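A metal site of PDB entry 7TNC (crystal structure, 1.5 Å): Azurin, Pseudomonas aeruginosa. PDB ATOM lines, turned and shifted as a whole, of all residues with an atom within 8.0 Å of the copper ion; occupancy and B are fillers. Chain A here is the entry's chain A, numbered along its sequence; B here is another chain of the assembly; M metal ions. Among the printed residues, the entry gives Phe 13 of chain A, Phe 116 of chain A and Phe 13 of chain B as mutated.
Gly 45 touches the copper ion (O to CU, 3.0 Å).
Phe 114 touches the copper ion (CB to CU, 3.8 Å).
Met 121 touches the copper ion.
Six residues have an atom within 4 Å of the copper ion: Gly 45, His 46, Cys 112, Phe 114, His 117 and Met 121.
Along chain A the residues within 4 Å of the copper ion span positions 45 to 121.
The nearest printed residue that does not touch the copper ion is Asn 47 (4.7 Å).
The backbone carbonyl oxygen (O) of Gly 45 lies close to a ring nitrogen (ND1) of His 117.
SG of Cys 112 sits close to N of Phe 114 (3.4 Å).
The side-chain sulfur (SD) of Met 121 sits close to a ring nitrogen (ND1) of His 46 (3.2 Å).
A ring nitrogen (NE2) of His 46 sits at hydrogen-bond distance from the backbone carbonyl oxygen (O) of Asn 10, 2.8 Å away.
N of Asn 47 sits close to SG of Cys 112, at 3.5 Å.
SD of Met 44 sits close to NE2 of His 117, 3.8 Å away.
The side-chain sulfur (SD) of Met 121 sits close to a ring nitrogen (ND1) of His 117, 3.7 Å away.
The backbone carbonyl oxygen (O) of His 46 is in hydrogen-bond range of the backbone NH (N) of Ile 87.
ND1 of His 46 binds the copper ion (2.0 Å).
ND1 of His 117 is bound to the copper ion (2.0 Å).
SG of Cys 112 is bound to the copper ion.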
ATOM      1  N   GLY A   9     -17.235  15.655  14.450  1.00  0.00           N
ATOM      2  CA  GLY A   9     -17.924  14.778  13.521  1.00  0.00           C
ATOM      3  C   GLY A   9     -18.397  13.581  14.302  1.00  0.00           C
ATOM      4  O   GLY A   9     -17.656  13.034  15.125  1.00  0.00           O
ATOM      5  N   ASN A  10     -19.639  13.143  14.081  1.00  0.00           N
ATOM      6  CA  ASN A  10     -20.244  12.133  14.934  1.00  0.00           C
ATOM      7  C   ASN A  10     -20.560  10.854  14.123  1.00  0.00           C
ATOM      8  O   ASN A  10     -20.159  10.706  12.977  1.00  0.00           O
ATOM      9  CB  ASN A  10     -21.466  12.699  15.674  1.00  0.00           C
ATOM     10  CG  ASN A  10     -22.580  13.087  14.732  1.00  0.00           C
ATOM     11  OD1 ASN A  10     -22.542  12.780  13.542  1.00  0.00           O
ATOM     12  ND2 ASN A  10     -23.602  13.768  15.277  1.00  0.00           N
ATOM     13  N   PHE A  13     -23.035  11.119  10.484  1.00  0.00           N
ATOM     14  CA  PHE A  13     -22.642  11.718   9.217  1.00  0.00           C
ATOM     15  C   PHE A  13     -22.670  13.247   9.266  1.00  0.00           C
ATOM     16  O   PHE A  13     -22.907  13.903   8.257  1.00  0.00           O
ATOM     17  CB  PHE A  13     -23.498  11.232   8.037  1.00  0.00           C
ATOM     18  CG  PHE A  13     -23.633   9.717   7.943  1.00  0.00           C
ATOM     19  CD1 PHE A  13     -22.617   8.938   7.410  1.00  0.00           C
ATOM     20  CD2 PHE A  13     -24.788   9.079   8.411  1.00  0.00           C
ATOM     21  CE1 PHE A  13     -22.743   7.558   7.310  1.00  0.00           C
ATOM     22  CE2 PHE A  13     -24.917   7.711   8.338  1.00  0.00           C
ATOM     23  CZ  PHE A  13     -23.887   6.941   7.776  1.00  0.00           C
ATOM     24  N   GLN A  14     -22.400  13.841  10.446  1.00  0.00           N
ATOM     25  CA  GLN A  14     -22.597  15.275  10.602  1.00  0.00           C
ATOM     26  C   GLN A  14     -21.406  15.941  11.256  1.00  0.00           C
ATOM     27  O   GLN A  14     -20.850  15.422  12.231  1.00  0.00           O
ATOM     28  CB  GLN A  14     -23.805  15.564  11.506  1.00  0.00           C
ATOM     29  CG  GLN A  14     -25.162  15.149  10.959  1.00  0.00           C
ATOM     30  CD  GLN A  14     -26.221  15.196  12.033  1.00  0.00           C
ATOM     31  OE1 GLN A  14     -25.948  14.926  13.210  1.00  0.00           O
ATOM     32  NE2 GLN A  14     -27.448  15.553  11.644  1.00  0.00           N
ATOM     33  N   PHE A  15     -21.035  17.109  10.741  1.00  0.00           N
ATOM     34  CA  PHE A  15     -20.276  18.086  11.516  1.00  0.00           C
ATOM     35  C   PHE A  15     -21.275  18.930  12.311  1.00  0.00           C
ATOM     36  O   PHE A  15     -22.455  19.030  11.970  1.00  0.00           O
ATOM     37  CB  PHE A  15     -19.562  19.078  10.605  1.00  0.00           C
ATOM     38  CG  PHE A  15     -18.303  18.565   9.918  1.00  0.00           C
ATOM     39  CD1 PHE A  15     -17.283  17.936  10.620  1.00  0.00           C
ATOM     40  CD2 PHE A  15     -18.145  18.774   8.571  1.00  0.00           C
ATOM     41  CE1 PHE A  15     -16.123  17.509   9.967  1.00  0.00           C
ATOM     42  CE2 PHE A  15     -17.003  18.337   7.910  1.00  0.00           C
ATOM     43  CZ  PHE A  15     -15.988  17.717   8.615  1.00  0.00           C
ATOM     44  N   LEU A  33     -10.613  19.358  15.769  1.00  0.00           N
ATOM     45  CA  LEU A  33     -11.596  18.351  15.401  1.00  0.00           C
ATOM     46  C   LEU A  33     -11.611  17.225  16.432  1.00  0.00           C
ATOM     47  O   LEU A  33     -10.555  16.770  16.874  1.00  0.00           O
ATOM     48  CB  LEU A  33     -11.273  17.791  14.022  1.00  0.00           C
ATOM     49  CG  LEU A  33     -12.281  16.770  13.501  1.00  0.00           C
ATOM     50  CD1 LEU A  33     -13.595  17.450  13.145  1.00  0.00           C
ATOM     51  CD2 LEU A  33     -11.705  16.100  12.265  1.00  0.00           C
ATOM     52  N   HIS A  35     -14.090  13.455  17.575  1.00  0.00           N
ATOM     53  CA  HIS A  35     -15.029  12.434  17.099  1.00  0.00           C
ATOM     54  C   HIS A  35     -15.692  11.845  18.341  1.00  0.00           C
ATOM     55  O   HIS A  35     -15.215  10.851  18.902  1.00  0.00           O
ATOM     56  CB  HIS A  35     -14.284  11.368  16.308  1.00  0.00           C
ATOM     57  CG  HIS A  35     -15.169  10.429  15.546  1.00  0.00           C
ATOM     58  ND1 HIS A  35     -16.331   9.912  16.079  1.00  0.00           N
ATOM     59  CD2 HIS A  35     -15.056   9.930  14.295  1.00  0.00           C
ATOM     60  CE1 HIS A  35     -16.892   9.107  15.182  1.00  0.00           C
ATOM     61  NE2 HIS A  35     -16.142   9.100  14.099  1.00  0.00           N
ATOM     62  N   VAL A  43     -14.879   2.668   9.399  1.00  0.00           N
ATOM     63  CA  VAL A  43     -16.274   2.737   8.973  1.00  0.00           C
ATOM     64  C   VAL A  43     -16.874   4.134   9.126  1.00  0.00           C
ATOM     65  O   VAL A  43     -17.849   4.447   8.428  1.00  0.00           O
ATOM     66  CB  VAL A  43     -17.168   1.703   9.702  1.00  0.00           C
ATOM     67  CG1 VAL A  43     -16.762   0.261   9.352  1.00  0.00           C
ATOM     68  CG2 VAL A  43     -17.189   1.923  11.183  1.00  0.00           C
ATOM     69  N   MET A  44     -16.332   4.987  10.003  1.00  0.00           N
ATOM     70  CA  MET A  44     -16.908   6.299  10.273  1.00  0.00           C
ATOM     71  C   MET A  44     -15.799   7.301  10.579  1.00  0.00           C
ATOM     72  O   MET A  44     -15.918   8.137  11.481  1.00  0.00           O
ATOM     73  CB  MET A  44     -17.926   6.230  11.414  1.00  0.00           C
ATOM     74  CG  MET A  44     -18.782   7.496  11.595  1.00  0.00           C
ATOM     75  SD  MET A  44     -19.910   7.843  10.219  1.00  0.00           S
ATOM     76  CE  MET A  44     -20.908   6.365  10.094  1.00  0.00           C
ATOM     77  N   GLY A  45     -14.700   7.216   9.835  1.00  0.00           N
ATOM     78  CA  GLY A  45     -13.632   8.199  10.003  1.00  0.00           C
ATOM     79  C   GLY A  45     -14.035   9.563   9.495  1.00  0.00           C
ATOM     80  O   GLY A  45     -14.795   9.705   8.547  1.00  0.00           O
ATOM     81  N   HIS A  46     -13.499  10.624  10.145  1.00  0.00           N
ATOM     82  CA  HIS A  46     -13.717  11.994   9.671  1.00  0.00           C
ATOM     83  C   HIS A  46     -12.422  12.766   9.641  1.00  0.00           C
ATOM     84  O   HIS A  46     -11.551  12.594  10.505  1.00  0.00           O
ATOM     85  CB  HIS A  46     -14.676  12.771  10.566  1.00  0.00           C
ATOM     86  CG  HIS A  46     -16.018  12.130  10.752  1.00  0.00           C
ATOM     87  ND1 HIS A  46     -16.821  11.782   9.690  1.00  0.00           N
ATOM     88  CD2 HIS A  46     -16.686  11.782  11.868  1.00  0.00           C
ATOM     89  CE1 HIS A  46     -17.935  11.237  10.156  1.00  0.00           C
ATOM     90  NE2 HIS A  46     -17.882  11.231  11.474  1.00  0.00           N
ATOM     91  N   ASN A  47     -12.308  13.644   8.662  1.00  0.00           N
ATOM     92  CA  ASN A  47     -11.291  14.679   8.689  1.00  0.00           C
ATOM     93  C   ASN A  47     -11.958  16.014   8.405  1.00  0.00           C
ATOM     94  O   ASN A  47     -13.157  16.099   8.098  1.00  0.00           O
ATOM     95  CB  ASN A  47     -10.145  14.355   7.712  1.00  0.00           C
ATOM     96  CG  ASN A  47     -10.629  14.090   6.295  1.00  0.00           C
ATOM     97  OD1 ASN A  47     -11.739  14.461   5.905  1.00  0.00           O
ATOM     98  ND2 ASN A  47      -9.787  13.401   5.519  1.00  0.00           N
ATOM     99  N   TRP A  48     -11.174  17.073   8.520  1.00  0.00           N
ATOM    100  CA  TRP A  48     -11.608  18.420   8.183  1.00  0.00           C
ATOM    101  C   TRP A  48     -10.618  18.934   7.148  1.00  0.00           C
ATOM    102  O   TRP A  48      -9.417  19.011   7.436  1.00  0.00           O
ATOM    103  CB  TRP A  48     -11.607  19.315   9.431  1.00  0.00           C
ATOM    104  CG  TRP A  48     -12.110  20.680   9.154  1.00  0.00           C
ATOM    105  CD1 TRP A  48     -13.397  21.108   9.249  1.00  0.00           C
ATOM    106  CD2 TRP A  48     -11.339  21.843   8.764  1.00  0.00           C
ATOM    107  NE1 TRP A  48     -13.498  22.438   8.935  1.00  0.00           N
ATOM    108  CE2 TRP A  48     -12.244  22.919   8.628  1.00  0.00           C
ATOM    109  CE3 TRP A  48      -9.979  22.063   8.519  1.00  0.00           C
ATOM    110  CZ2 TRP A  48     -11.841  24.201   8.254  1.00  0.00           C
ATOM    111  CZ3 TRP A  48      -9.578  23.336   8.135  1.00  0.00           C
ATOM    112  CH2 TRP A  48     -10.500  24.384   8.005  1.00  0.00           C
ATOM    113  N   LEU A  86      -7.310  12.055   9.571  1.00  0.00           N
ATOM    114  CA  LEU A  86      -8.567  11.312   9.711  1.00  0.00           C
ATOM    115  C   LEU A  86      -8.621  10.675  11.085  1.00  0.00           C
ATOM    116  O   LEU A  86      -7.652  10.039  11.519  1.00  0.00           O
ATOM    117  CB  LEU A  86      -8.650  10.240   8.629  1.00  0.00           C
ATOM    118  CG  LEU A  86     -10.004   9.529   8.453  1.00  0.00           C
ATOM    119  CD1 LEU A  86     -10.890  10.353   7.533  1.00  0.00           C
ATOM    120  CD2 LEU A  86      -9.768   8.126   7.896  1.00  0.00           C
ATOM    121  N   ILE A  87      -9.752  10.832  11.791  1.00  0.00           N
ATOM    122  CA  ILE A  87      -9.905  10.330  13.147  1.00  0.00           C
ATOM    123  C   ILE A  87     -11.159   9.469  13.238  1.00  0.00           C
ATOM    124  O   ILE A  87     -12.128   9.632  12.481  1.00  0.00           O
ATOM    125  CB  ILE A  87      -9.941  11.466  14.190  1.00  0.00           C
ATOM    126  CG1 ILE A  87     -11.070  12.455  13.906  1.00  0.00           C
ATOM    127  CG2 ILE A  87      -8.601  12.197  14.209  1.00  0.00           C
ATOM    128  CD1 ILE A  87     -11.275  13.503  15.013  1.00  0.00           C
ATOM    129  N   PHE A 111     -14.842  20.279   4.406  1.00  0.00           N
ATOM    130  CA  PHE A 111     -15.570  19.030   4.166  1.00  0.00           C
ATOM    131  C   PHE A 111     -14.746  17.872   4.697  1.00  0.00           C
ATOM    132  O   PHE A 111     -13.549  18.008   4.991  1.00  0.00           O
ATOM    133  CB  PHE A 111     -15.848  18.849   2.665  1.00  0.00           C
ATOM    134  CG  PHE A 111     -14.657  19.135   1.791  1.00  0.00           C
ATOM    135  CD1 PHE A 111     -13.737  18.132   1.514  1.00  0.00           C
ATOM    136  CD2 PHE A 111     -14.435  20.411   1.270  1.00  0.00           C
ATOM    137  CE1 PHE A 111     -12.606  18.392   0.728  1.00  0.00           C
ATOM    138  CE2 PHE A 111     -13.315  20.672   0.494  1.00  0.00           C
ATOM    139  CZ  PHE A 111     -12.419  19.654   0.214  1.00  0.00           C
ATOM    140  N   CYS A 112     -15.407  16.719   4.844  1.00  0.00           N
ATOM    141  CA  CYS A 112     -14.738  15.466   5.179  1.00  0.00           C
ATOM    142  C   CYS A 112     -14.596  14.671   3.889  1.00  0.00           C
ATOM    143  O   CYS A 112     -15.509  14.667   3.043  1.00  0.00           O
ATOM    144  CB  CYS A 112     -15.574  14.695   6.189  1.00  0.00           C
ATOM    145  SG  CYS A 112     -14.982  13.047   6.492  1.00  0.00           S
ATOM    146  N   THR A 113     -13.459  13.988   3.707  1.00  0.00           N
ATOM    147  CA  THR A 113     -13.210  13.226   2.477  1.00  0.00           C
ATOM    148  C   THR A 113     -13.405  11.725   2.643  1.00  0.00           C
ATOM    149  O   THR A 113     -13.169  10.979   1.684  1.00  0.00           O
ATOM    150  CB  THR A 113     -11.830  13.527   1.865  1.00  0.00           C
ATOM    151  OG1 THR A 113     -10.796  13.139   2.770  1.00  0.00           O
ATOM    152  CG2 THR A 113     -11.731  15.003   1.489  1.00  0.00           C
ATOM    153  N   PHE A 114     -13.837  11.271   3.808  1.00  0.00           N
ATOM    154  CA  PHE A 114     -14.189   9.866   3.951  1.00  0.00           C
ATOM    155  C   PHE A 114     -15.299   9.530   2.951  1.00  0.00           C
ATOM    156  O   PHE A 114     -16.226  10.339   2.777  1.00  0.00           O
ATOM    157  CB  PHE A 114     -14.673   9.590   5.365  1.00  0.00           C
ATOM    158  CG  PHE A 114     -14.882   8.146   5.644  1.00  0.00           C
ATOM    159  CD1 PHE A 114     -16.077   7.529   5.317  1.00  0.00           C
ATOM    160  CD2 PHE A 114     -13.876   7.390   6.205  1.00  0.00           C
ATOM    161  CE1 PHE A 114     -16.268   6.177   5.589  1.00  0.00           C
ATOM    162  CE2 PHE A 114     -14.044   6.044   6.469  1.00  0.00           C
ATOM    163  CZ  PHE A 114     -15.245   5.434   6.145  1.00  0.00           C
ATOM    164  N   PRO A 115     -15.235   8.370   2.274  1.00  0.00           N
ATOM    165  CA  PRO A 115     -16.206   8.078   1.206  1.00  0.00           C
ATOM    166  C   PRO A 115     -17.655   8.434   1.520  1.00  0.00           C
ATOM    167  O   PRO A 115     -18.236   7.968   2.509  1.00  0.00           O
ATOM    168  CB  PRO A 115     -16.025   6.574   0.981  1.00  0.00           C
ATOM    169  CG  PRO A 115     -14.552   6.362   1.265  1.00  0.00           C
ATOM    170  CD  PRO A 115     -14.257   7.279   2.442  1.00  0.00           C
ATOM    171  N   PHE A 116     -18.173   9.325   0.686  1.00  0.00           N
ATOM    172  CA  PHE A 116     -19.571   9.746   0.596  1.00  0.00           C
ATOM    173  C   PHE A 116     -19.950  10.772   1.663  1.00  0.00           C
ATOM    174  O   PHE A 116     -20.991  11.418   1.542  1.00  0.00           O
ATOM    175  CB  PHE A 116     -20.551   8.573   0.561  1.00  0.00           C
ATOM    176  CG  PHE A 116     -20.278   7.635  -0.576  1.00  0.00           C
ATOM    177  CD1 PHE A 116     -20.448   8.059  -1.892  1.00  0.00           C
ATOM    178  CD2 PHE A 116     -19.709   6.388  -0.355  1.00  0.00           C
ATOM    179  CE1 PHE A 116     -20.157   7.214  -2.953  1.00  0.00           C
ATOM    180  CE2 PHE A 116     -19.412   5.545  -1.408  1.00  0.00           C
ATOM    181  CZ  PHE A 116     -19.627   5.958  -2.708  1.00  0.00           C
ATOM    182  N   HIS A 117     -19.131  10.978   2.695  1.00  0.00           N
ATOM    183  CA  HIS A 117     -19.546  11.856   3.782  1.00  0.00           C
ATOM    184  C   HIS A 117     -19.770  13.298   3.341  1.00  0.00           C
ATOM    185  O   HIS A 117     -20.586  13.998   3.953  1.00  0.00           O
ATOM    186  CB  HIS A 117     -18.517  11.856   4.907  1.00  0.00           C
ATOM    187  CG  HIS A 117     -18.522  10.622   5.757  1.00  0.00           C
ATOM    188  ND1 HIS A 117     -17.713  10.483   6.866  1.00  0.00           N
ATOM    189  CD2 HIS A 117     -19.215   9.470   5.644  1.00  0.00           C
ATOM    190  CE1 HIS A 117     -17.929   9.300   7.418  1.00  0.00           C
ATOM    191  NE2 HIS A 117     -18.842   8.671   6.692  1.00  0.00           N
ATOM    192  N   SER A 118     -19.028  13.775   2.338  1.00  0.00           N
ATOM    193  CA  SER A 118     -19.060  15.207   2.037  1.00  0.00           C
ATOM    194  C   SER A 118     -20.432  15.688   1.580  1.00  0.00           C
ATOM    195  O   SER A 118     -20.685  16.897   1.611  1.00  0.00           O
ATOM    196  CB  SER A 118     -17.999  15.555   0.996  1.00  0.00           C
ATOM    197  OG  SER A 118     -18.437  15.169  -0.302  1.00  0.00           O
ATOM    198  N   MET A 121     -21.351  16.337   5.223  1.00  0.00           N
ATOM    199  CA  MET A 121     -20.245  16.900   6.016  1.00  0.00           C
ATOM    200  C   MET A 121     -19.469  17.928   5.179  1.00  0.00           C
ATOM    201  O   MET A 121     -18.398  17.641   4.623  1.00  0.00           O
ATOM    202  CB  MET A 121     -19.347  15.789   6.525  1.00  0.00           C
ATOM    203  CG  MET A 121     -20.099  14.688   7.244  1.00  0.00           C
ATOM    204  SD  MET A 121     -19.094  13.599   8.283  1.00  0.00           S
ATOM    205  CE  MET A 121     -18.294  14.778   9.396  1.00  0.00           C
ATOM    206  N   PHE B  13     -27.721  11.036   3.383  1.00  0.00           N
ATOM    207  CA  PHE B  13     -27.947  10.186   4.543  1.00  0.00           C
ATOM    208  C   PHE B  13     -29.203  10.587   5.319  1.00  0.00           C
ATOM    209  O   PHE B  13     -29.279  10.402   6.529  1.00  0.00           O
ATOM    210  CB  PHE B  13     -26.746  10.154   5.502  1.00  0.00           C
ATOM    211  CG  PHE B  13     -25.411   9.866   4.824  1.00  0.00           C
ATOM    212  CD1 PHE B  13     -25.049   8.575   4.473  1.00  0.00           C
ATOM    213  CD2 PHE B  13     -24.527  10.912   4.531  1.00  0.00           C
ATOM    214  CE1 PHE B  13     -23.826   8.308   3.869  1.00  0.00           C
ATOM    215  CE2 PHE B  13     -23.323  10.664   3.913  1.00  0.00           C
ATOM    216  CZ  PHE B  13     -22.964   9.348   3.584  1.00  0.00           C
HETATM  217 CU    CU M   1     -16.541  11.930   7.690  1.00  0.00          CU
